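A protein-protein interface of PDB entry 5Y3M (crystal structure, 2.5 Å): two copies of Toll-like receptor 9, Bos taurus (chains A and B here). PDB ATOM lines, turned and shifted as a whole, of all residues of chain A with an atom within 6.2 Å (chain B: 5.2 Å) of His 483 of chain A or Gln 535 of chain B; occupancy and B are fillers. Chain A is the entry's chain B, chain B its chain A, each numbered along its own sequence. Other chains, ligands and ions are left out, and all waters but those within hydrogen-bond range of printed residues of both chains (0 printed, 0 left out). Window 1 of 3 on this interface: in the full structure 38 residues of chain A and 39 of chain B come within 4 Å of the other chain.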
ATOM      1  N   ASP A 403     -26.546  -7.902  33.002  1.00  0.00           N
ATOM      2  CA  ASP A 403     -25.636  -6.773  33.256  1.00  0.00           C
ATOM      3  C   ASP A 403     -24.857  -6.943  34.570  1.00  0.00           C
ATOM      4  O   ASP A 403     -24.806  -6.052  35.409  1.00  0.00           O
ATOM      5  CB  ASP A 403     -26.390  -5.433  33.202  1.00  0.00           C
ATOM      6  CG  ASP A 403     -26.713  -4.999  31.773  1.00  0.00           C
ATOM      7  OD1 ASP A 403     -25.765  -4.779  30.984  1.00  0.00           O
ATOM      8  OD2 ASP A 403     -27.912  -4.865  31.443  1.00  0.00           O
ATOM      9  N   ASN A 404     -24.264  -8.118  34.729  1.00  0.00           N
ATOM     10  CA  ASN A 404     -23.395  -8.426  35.861  1.00  0.00           C
ATOM     11  C   ASN A 404     -22.010  -8.780  35.298  1.00  0.00           C
ATOM     12  O   ASN A 404     -21.754  -8.536  34.116  1.00  0.00           O
ATOM     13  CB  ASN A 404     -24.018  -9.565  36.691  1.00  0.00           C
ATOM     14  CG  ASN A 404     -25.111  -9.086  37.621  1.00  0.00           C
ATOM     15  OD1 ASN A 404     -26.264  -9.515  37.521  1.00  0.00           O
ATOM     16  ND2 ASN A 404     -24.757  -8.205  38.534  1.00  0.00           N
ATOM     17  N   SER A 458     -27.962 -12.459  30.373  1.00  0.00           N
ATOM     18  CA  SER A 458     -27.431 -11.688  29.262  1.00  0.00           C
ATOM     19  C   SER A 458     -26.523 -10.572  29.785  1.00  0.00           C
ATOM     20  O   SER A 458     -26.646 -10.162  30.936  1.00  0.00           O
ATOM     21  CB  SER A 458     -28.573 -11.108  28.421  1.00  0.00           C
ATOM     22  OG  SER A 458     -29.345 -10.193  29.188  1.00  0.00           O
ATOM     23  N   ARG A 459     -25.603 -10.108  28.939  1.00  0.00           N
ATOM     24  CA  ARG A 459     -24.667  -9.027  29.286  1.00  0.00           C
ATOM     25  C   ARG A 459     -23.797  -9.357  30.515  1.00  0.00           C
ATOM     26  O   ARG A 459     -23.660  -8.557  31.444  1.00  0.00           O
ATOM     27  CB  ARG A 459     -25.409  -7.686  29.435  1.00  0.00           C
ATOM     28  CG  ARG A 459     -26.103  -7.240  28.161  1.00  0.00           C
ATOM     29  CD  ARG A 459     -27.244  -6.268  28.420  1.00  0.00           C
ATOM     30  NE  ARG A 459     -28.082  -6.150  27.224  1.00  0.00           N
ATOM     31  CZ  ARG A 459     -27.946  -5.229  26.260  1.00  0.00           C
ATOM     32  NH1 ARG A 459     -27.004  -4.268  26.309  1.00  0.00           N
ATOM     33  NH2 ARG A 459     -28.784  -5.265  25.219  1.00  0.00           N
ATOM     34  N   ASN A 460     -23.212 -10.552  30.483  1.00  0.00           N
ATOM     35  CA  ASN A 460     -22.268 -11.031  31.495  1.00  0.00           C
ATOM     36  C   ASN A 460     -20.954 -11.405  30.809  1.00  0.00           C
ATOM     37  O   ASN A 460     -20.826 -11.208  29.605  1.00  0.00           O
ATOM     38  CB  ASN A 460     -22.887 -12.214  32.243  1.00  0.00           C
ATOM     39  CG  ASN A 460     -23.747 -11.768  33.409  1.00  0.00           C
ATOM     40  OD1 ASN A 460     -23.247 -11.580  34.514  1.00  0.00           O
ATOM     41  ND2 ASN A 460     -25.043 -11.598  33.167  1.00  0.00           N
ATOM     42  N   ASN A 461     -19.981 -11.927  31.561  1.00  0.00           N
ATOM     43  CA  ASN A 461     -18.643 -12.243  31.017  1.00  0.00           C
ATOM     44  C   ASN A 461     -18.355 -13.737  30.812  1.00  0.00           C
ATOM     45  O   ASN A 461     -17.211 -14.188  30.985  1.00  0.00           O
ATOM     46  CB  ASN A 461     -17.563 -11.622  31.915  1.00  0.00           C
ATOM     47  CG  ASN A 461     -17.689 -10.113  32.015  1.00  0.00           C
ATOM     48  OD1 ASN A 461     -18.216  -9.458  31.114  1.00  0.00           O
ATOM     49  ND2 ASN A 461     -17.196  -9.553  33.110  1.00  0.00           N
ATOM     50  N   LEU A 481     -28.804 -15.908  27.201  1.00  0.00           N
ATOM     51  CA  LEU A 481     -27.351 -15.745  27.324  1.00  0.00           C
ATOM     52  C   LEU A 481     -26.808 -14.768  26.272  1.00  0.00           C
ATOM     53  O   LEU A 481     -25.640 -14.852  25.880  1.00  0.00           O
ATOM     54  CB  LEU A 481     -26.640 -17.104  27.194  1.00  0.00           C
ATOM     55  CG  LEU A 481     -26.786 -18.101  28.339  1.00  0.00           C
ATOM     56  CD1 LEU A 481     -26.191 -19.446  27.943  1.00  0.00           C
ATOM     57  CD2 LEU A 481     -26.108 -17.590  29.595  1.00  0.00           C
ATOM     58  N   SER A 482     -27.640 -13.823  25.839  1.00  0.00           N
ATOM     59  CA  SER A 482     -27.237 -12.889  24.794  1.00  0.00           C
ATOM     60  C   SER A 482     -26.242 -11.856  25.315  1.00  0.00           C
ATOM     61  O   SER A 482     -26.158 -11.610  26.513  1.00  0.00           O
ATOM     62  CB  SER A 482     -28.446 -12.188  24.165  1.00  0.00           C
ATOM     63  OG  SER A 482     -28.975 -11.188  25.016  1.00  0.00           O
ATOM     64  N   HIS A 483     -25.469 -11.278  24.398  1.00  0.00           N
ATOM     65  CA  HIS A 483     -24.502 -10.222  24.720  1.00  0.00           C
ATOM     66  C   HIS A 483     -23.491 -10.662  25.792  1.00  0.00           C
ATOM     67  O   HIS A 483     -23.071  -9.867  26.638  1.00  0.00           O
ATOM     68  CB  HIS A 483     -25.214  -8.927  25.140  1.00  0.00           C
ATOM     69  CG  HIS A 483     -25.992  -8.277  24.041  1.00  0.00           C
ATOM     70  ND1 HIS A 483     -27.357  -8.417  23.913  1.00  0.00           N
ATOM     71  CD2 HIS A 483     -25.599  -7.463  23.032  1.00  0.00           C
ATOM     72  CE1 HIS A 483     -27.773  -7.723  22.869  1.00  0.00           C
ATOM     73  NE2 HIS A 483     -26.727  -7.134  22.317  1.00  0.00           N
ATOM     74  N   ASN A 484     -23.104 -11.936  25.743  1.00  0.00           N
ATOM     75  CA  ASN A 484     -22.008 -12.455  26.551  1.00  0.00           C
ATOM     76  C   ASN A 484     -20.777 -12.478  25.645  1.00  0.00           C
ATOM     77  O   ASN A 484     -20.768 -11.821  24.603  1.00  0.00           O
ATOM     78  CB  ASN A 484     -22.372 -13.832  27.125  1.00  0.00           C
ATOM     79  CG  ASN A 484     -23.061 -13.734  28.470  1.00  0.00           C
ATOM     80  OD1 ASN A 484     -22.415 -13.841  29.511  1.00  0.00           O
ATOM     81  ND2 ASN A 484     -24.373 -13.516  28.457  1.00  0.00           N
ATOM     82  N   SER A 485     -19.729 -13.194  26.042  1.00  0.00           N
ATOM     83  CA  SER A 485     -18.520 -13.321  25.229  1.00  0.00           C
ATOM     84  C   SER A 485     -18.192 -14.775  24.904  1.00  0.00           C
ATOM     85  O   SER A 485     -17.024 -15.155  24.813  1.00  0.00           O
ATOM     86  CB  SER A 485     -17.379 -12.665  25.985  1.00  0.00           C
ATOM     87  OG  SER A 485     -17.666 -11.296  26.167  1.00  0.00           O
ATOM     88  N   LEU A 506     -28.768 -17.196  22.399  1.00  0.00           N
ATOM     89  CA  LEU A 506     -27.309 -17.044  22.399  1.00  0.00           C
ATOM     90  C   LEU A 506     -26.826 -15.957  21.418  1.00  0.00           C
ATOM     91  O   LEU A 506     -25.700 -16.021  20.907  1.00  0.00           O
ATOM     92  CB  LEU A 506     -26.655 -18.396  22.087  1.00  0.00           C
ATOM     93  CG  LEU A 506     -26.639 -19.367  23.268  1.00  0.00           C
ATOM     94  CD1 LEU A 506     -26.501 -20.799  22.782  1.00  0.00           C
ATOM     95  CD2 LEU A 506     -25.527 -19.021  24.254  1.00  0.00           C
ATOM     96  N   SER A 507     -27.660 -14.940  21.188  1.00  0.00           N
ATOM     97  CA  SER A 507     -27.320 -13.861  20.258  1.00  0.00           C
ATOM     98  C   SER A 507     -26.211 -12.965  20.812  1.00  0.00           C
ATOM     99  O   SER A 507     -26.010 -12.902  22.014  1.00  0.00           O
ATOM    100  CB  SER A 507     -28.553 -13.021  19.911  1.00  0.00           C
ATOM    101  OG  SER A 507     -29.163 -12.476  21.071  1.00  0.00           O
ATOM    102  N   HIS A 508     -25.485 -12.300  19.920  1.00  0.00           N
ATOM    103  CA  HIS A 508     -24.384 -11.403  20.296  1.00  0.00           C
ATOM    104  C   HIS A 508     -23.334 -12.125  21.167  1.00  0.00           C
ATOM    105  O   HIS A 508     -23.006 -11.704  22.274  1.00  0.00           O
ATOM    106  CB  HIS A 508     -24.902 -10.109  20.952  1.00  0.00           C
ATOM    107  CG  HIS A 508     -25.775  -9.277  20.059  1.00  0.00           C
ATOM    108  ND1 HIS A 508     -27.144  -9.438  19.991  1.00  0.00           N
ATOM    109  CD2 HIS A 508     -25.474  -8.266  19.208  1.00  0.00           C
ATOM    110  CE1 HIS A 508     -27.648  -8.568  19.132  1.00  0.00           C
ATOM    111  NE2 HIS A 508     -26.656  -7.847  18.641  1.00  0.00           N
ATOM    112  N   ASN A 509     -22.836 -13.235  20.633  1.00  0.00           N
ATOM    113  CA  ASN A 509     -21.762 -14.021  21.243  1.00  0.00           C
ATOM    114  C   ASN A 509     -20.736 -14.314  20.153  1.00  0.00           C
ATOM    115  O   ASN A 509     -20.741 -13.637  19.129  1.00  0.00           O
ATOM    116  CB  ASN A 509     -22.351 -15.285  21.879  1.00  0.00           C
ATOM    117  CG  ASN A 509     -22.904 -15.023  23.268  1.00  0.00           C
ATOM    118  OD1 ASN A 509     -22.141 -14.803  24.206  1.00  0.00           O
ATOM    119  ND2 ASN A 509     -24.230 -15.039  23.404  1.00  0.00           N
ATOM    120  N   LYS B 510     -15.780  -4.163  25.955  1.00  0.00           N
ATOM    121  CA  LYS B 510     -16.824  -3.759  26.909  1.00  0.00           C
ATOM    122  C   LYS B 510     -16.224  -3.005  28.098  1.00  0.00           C
ATOM    123  O   LYS B 510     -16.614  -3.227  29.248  1.00  0.00           O
ATOM    124  CB  LYS B 510     -17.602  -4.993  27.377  1.00  0.00           C
ATOM    125  CG  LYS B 510     -18.133  -5.837  26.225  1.00  0.00           C
ATOM    126  CD  LYS B 510     -18.994  -6.994  26.690  1.00  0.00           C
ATOM    127  CE  LYS B 510     -19.449  -7.826  25.500  1.00  0.00           C
ATOM    128  NZ  LYS B 510     -20.221  -9.017  25.940  1.00  0.00           N
ATOM    129  N   ASN B 533     -17.518   0.220  22.376  1.00  0.00           N
ATOM    130  CA  ASN B 533     -17.633  -0.238  23.766  1.00  0.00           C
ATOM    131  C   ASN B 533     -18.945   0.292  24.354  1.00  0.00           C
ATOM    132  O   ASN B 533     -18.951   0.981  25.379  1.00  0.00           O
ATOM    133  CB  ASN B 533     -16.453   0.276  24.602  1.00  0.00           C
ATOM    134  CG  ASN B 533     -15.125  -0.328  24.195  1.00  0.00           C
ATOM    135  OD1 ASN B 533     -14.484  -1.010  24.993  1.00  0.00           O
ATOM    136  ND2 ASN B 533     -14.695  -0.071  22.963  1.00  0.00           N
ATOM    137  N   SER B 534     -20.055  -0.033  23.698  1.00  0.00           N
ATOM    138  CA  SER B 534     -21.358   0.544  24.028  1.00  0.00           C
ATOM    139  C   SER B 534     -22.091  -0.107  25.202  1.00  0.00           C
ATOM    140  O   SER B 534     -22.870   0.569  25.885  1.00  0.00           O
ATOM    141  CB  SER B 534     -22.267   0.528  22.800  1.00  0.00           C
ATOM    142  OG  SER B 534     -22.604  -0.791  22.438  1.00  0.00           O
ATOM    143  N   GLN B 535     -21.865  -1.398  25.431  1.00  0.00           N
ATOM    144  CA  GLN B 535     -22.649  -2.163  26.421  1.00  0.00           C
ATOM    145  C   GLN B 535     -22.626  -1.551  27.828  1.00  0.00           C
ATOM    146  O   GLN B 535     -23.676  -1.448  28.464  1.00  0.00           O
ATOM    147  CB  GLN B 535     -22.227  -3.641  26.449  1.00  0.00           C
ATOM    148  CG  GLN B 535     -23.019  -4.527  27.404  1.00  0.00           C
ATOM    149  CD  GLN B 535     -22.639  -5.996  27.276  1.00  0.00           C
ATOM    150  OE1 GLN B 535     -22.631  -6.560  26.175  1.00  0.00           O
ATOM    151  NE2 GLN B 535     -22.308  -6.619  28.400  1.00  0.00           N
ATOM    152  N   PRO B 536     -21.443  -1.135  28.316  1.00  0.00           N
ATOM    153  CA  PRO B 536     -21.429  -0.447  29.612  1.00  0.00           C
ATOM    154  C   PRO B 536     -22.285   0.816  29.663  1.00  0.00           C
ATOM    155  O   PRO B 536     -22.939   1.056  30.670  1.00  0.00           O
ATOM    156  CB  PRO B 536     -19.948  -0.118  29.815  1.00  0.00           C
ATOM    157  CG  PRO B 536     -19.240  -1.203  29.076  1.00  0.00           C
ATOM    158  CD  PRO B 536     -20.075  -1.436  27.851  1.00  0.00           C
ATOM    159  N   PHE B 537     -22.299   1.598  28.581  1.00  0.00           N
ATOM    160  CA  PHE B 537     -23.123   2.819  28.506  1.00  0.00           C
ATOM    161  C   PHE B 537     -24.636   2.571  28.343  1.00  0.00           C
ATOM    162  O   PHE B 537     -25.412   3.519  28.398  1.00  0.00           O
ATOM    163  CB  PHE B 537     -22.627   3.721  27.369  1.00  0.00           C
ATOM    164  CG  PHE B 537     -21.283   4.363  27.631  1.00  0.00           C
ATOM    165  CD1 PHE B 537     -21.162   5.407  28.547  1.00  0.00           C
ATOM    166  CD2 PHE B 537     -20.144   3.941  26.946  1.00  0.00           C
ATOM    167  CE1 PHE B 537     -19.930   6.007  28.787  1.00  0.00           C
ATOM    168  CE2 PHE B 537     -18.910   4.538  27.179  1.00  0.00           C
ATOM    169  CZ  PHE B 537     -18.802   5.573  28.102  1.00  0.00           C
ATOM    170  N   SER B 538     -25.044   1.319  28.112  1.00  0.00           N
ATOM    171  CA  SER B 538     -26.463   0.909  28.110  1.00  0.00           C
ATOM    172  C   SER B 538     -26.951   0.349  29.456  1.00  0.00           C
ATOM    173  O   SER B 538     -28.087  -0.095  29.563  1.00  0.00           O
ATOM    174  CB  SER B 538     -26.710  -0.145  27.028  1.00  0.00           C
ATOM    175  OG  SER B 538     -26.431   0.372  25.741  1.00  0.00           O
ATOM    176  N   MET B 539     -26.092   0.365  30.474  1.00  0.00           N
ATOM    177  CA  MET B 539     -26.464  -0.078  31.811  1.00  0.00           C
ATOM    178  C   MET B 539     -27.258   1.036  32.499  1.00  0.00           C
ATOM    179  O   MET B 539     -26.686   1.950  33.098  1.00  0.00           O
ATOM    180  CB  MET B 539     -25.210  -0.470  32.609  1.00  0.00           C
ATOM    181  CG  MET B 539     -24.491  -1.693  32.048  1.00  0.00           C
ATOM    182  SD  MET B 539     -22.889  -2.039  32.794  1.00  0.00           S
ATOM    183  CE  MET B 539     -23.384  -2.514  34.448  1.00  0.00           C
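NZ of Lys 510 of chain B is in hydrogen-bond range of O of Asn 484 of chain A, 3.2 Å away.
OG of Ser 485 of chain A sits at hydrogen-bond distance from NZ of Lys 510 of chain B, at 3.4 Å.
The side-chain amino group (NZ) of Lys 510 of chain B lies within hydrogen-bond range of the backbone carbonyl oxygen (O) of His 483 of chain A.
The backbone carbonyl oxygen (O) of His 483 of chain A sits close to the side-chain amide oxygen (OE1) of Gln 535 of chain B (3.4 Å).
The backbone NH (N) of Asp 403 of chain A sits at hydrogen-bond distance from the backbone carbonyl oxygen (O) of Ser 458 of chain A (3.1 Å).
O of His 508 of chain A lies close to N of His 483 of chain A (3.3 Å).
The backbone NH (N) of Ser 485 of chain A is in hydrogen-bond range of the side-chain amide oxygen (OD1) of Asn 509 of chain A, 3.4 Å away.
The backbone NH (N) of Asn 484 of chain A lies within hydrogen-bond range of the backbone carbonyl oxygen (O) of His 508 of chain A, at 3.5 Å.
The backbone NH (N) of Arg 459 of chain A lies within hydrogen-bond range of the backbone carbonyl oxygen (O) of Ser 482 of chain A (2.9 Å).
The backbone carbonyl oxygen (O) of His 483 of chain A sits close to the backbone NH (N) of Arg 459 of chain A (3.4 Å).
Met 539 of chain B touches Asp 403 of chain A.
CB of Arg 459 of chain A touches NE2 of Gln 535 of chain B, at 3.4 Å.
Of chain B, only Lys 510 and Gln 535 come within 4 Å of His 483 of chain A.
Gln 535 of chain B touches just these residues of chain A: Arg 459 (3.4 Å) and His 483 (3.4 Å).
Printed residues of chain B within 4 Å of Ser 485 of chain A: Lys 510 (3.4 Å).
Of the printed residues of chain B, Asn 484 of chain A touches Lys 510 (3.2 Å).
Printed residues of chain B within 4 Å of Arg 459 of chain A: Gln 535.
Of the printed residues of chain A, Met 539 of chain B touches Asp 403 (3.5 Å).
Printed residues of chain B within 4 Å of Asp 403 of chain A: Met 539 (3.5 Å).
Ser 458 of chain A touches none of the printed residues of chain B.
Pro 536 of chain B touches none of the printed residues of chain A.
The nearest printed residue of chain A that does not touch Gln 535 of chain B is Asp 403 of chain A (4.5 Å).
The nearest printed residue of chain A that does not touch Lys 510 of chain B is Asn 460 of chain A (4.3 Å).
Of the 15 printed residues of chain A, 5 touch a printed residue of chain B.
Of the 8 printed residues of chain B, 3 touch a printed residue of chain A.
Printed residues of chain B that touch a printed residue of chain A: Lys 510, Gln 535 and Met 539.
Hydrophobic or aromatic side chains of chain B that line the printed part of chain A: Met 539.
Along chain B the printed residues that touch a printed residue of chain A span positions 510 to 539.
Among the printed residues, 6 pairs touch across the chains.
Among the printed residues, no Asp or Glu carboxylate lies within 4 Å of a Lys or Arg side-chain nitrogen of the other chain.
No position is printed for both chains.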
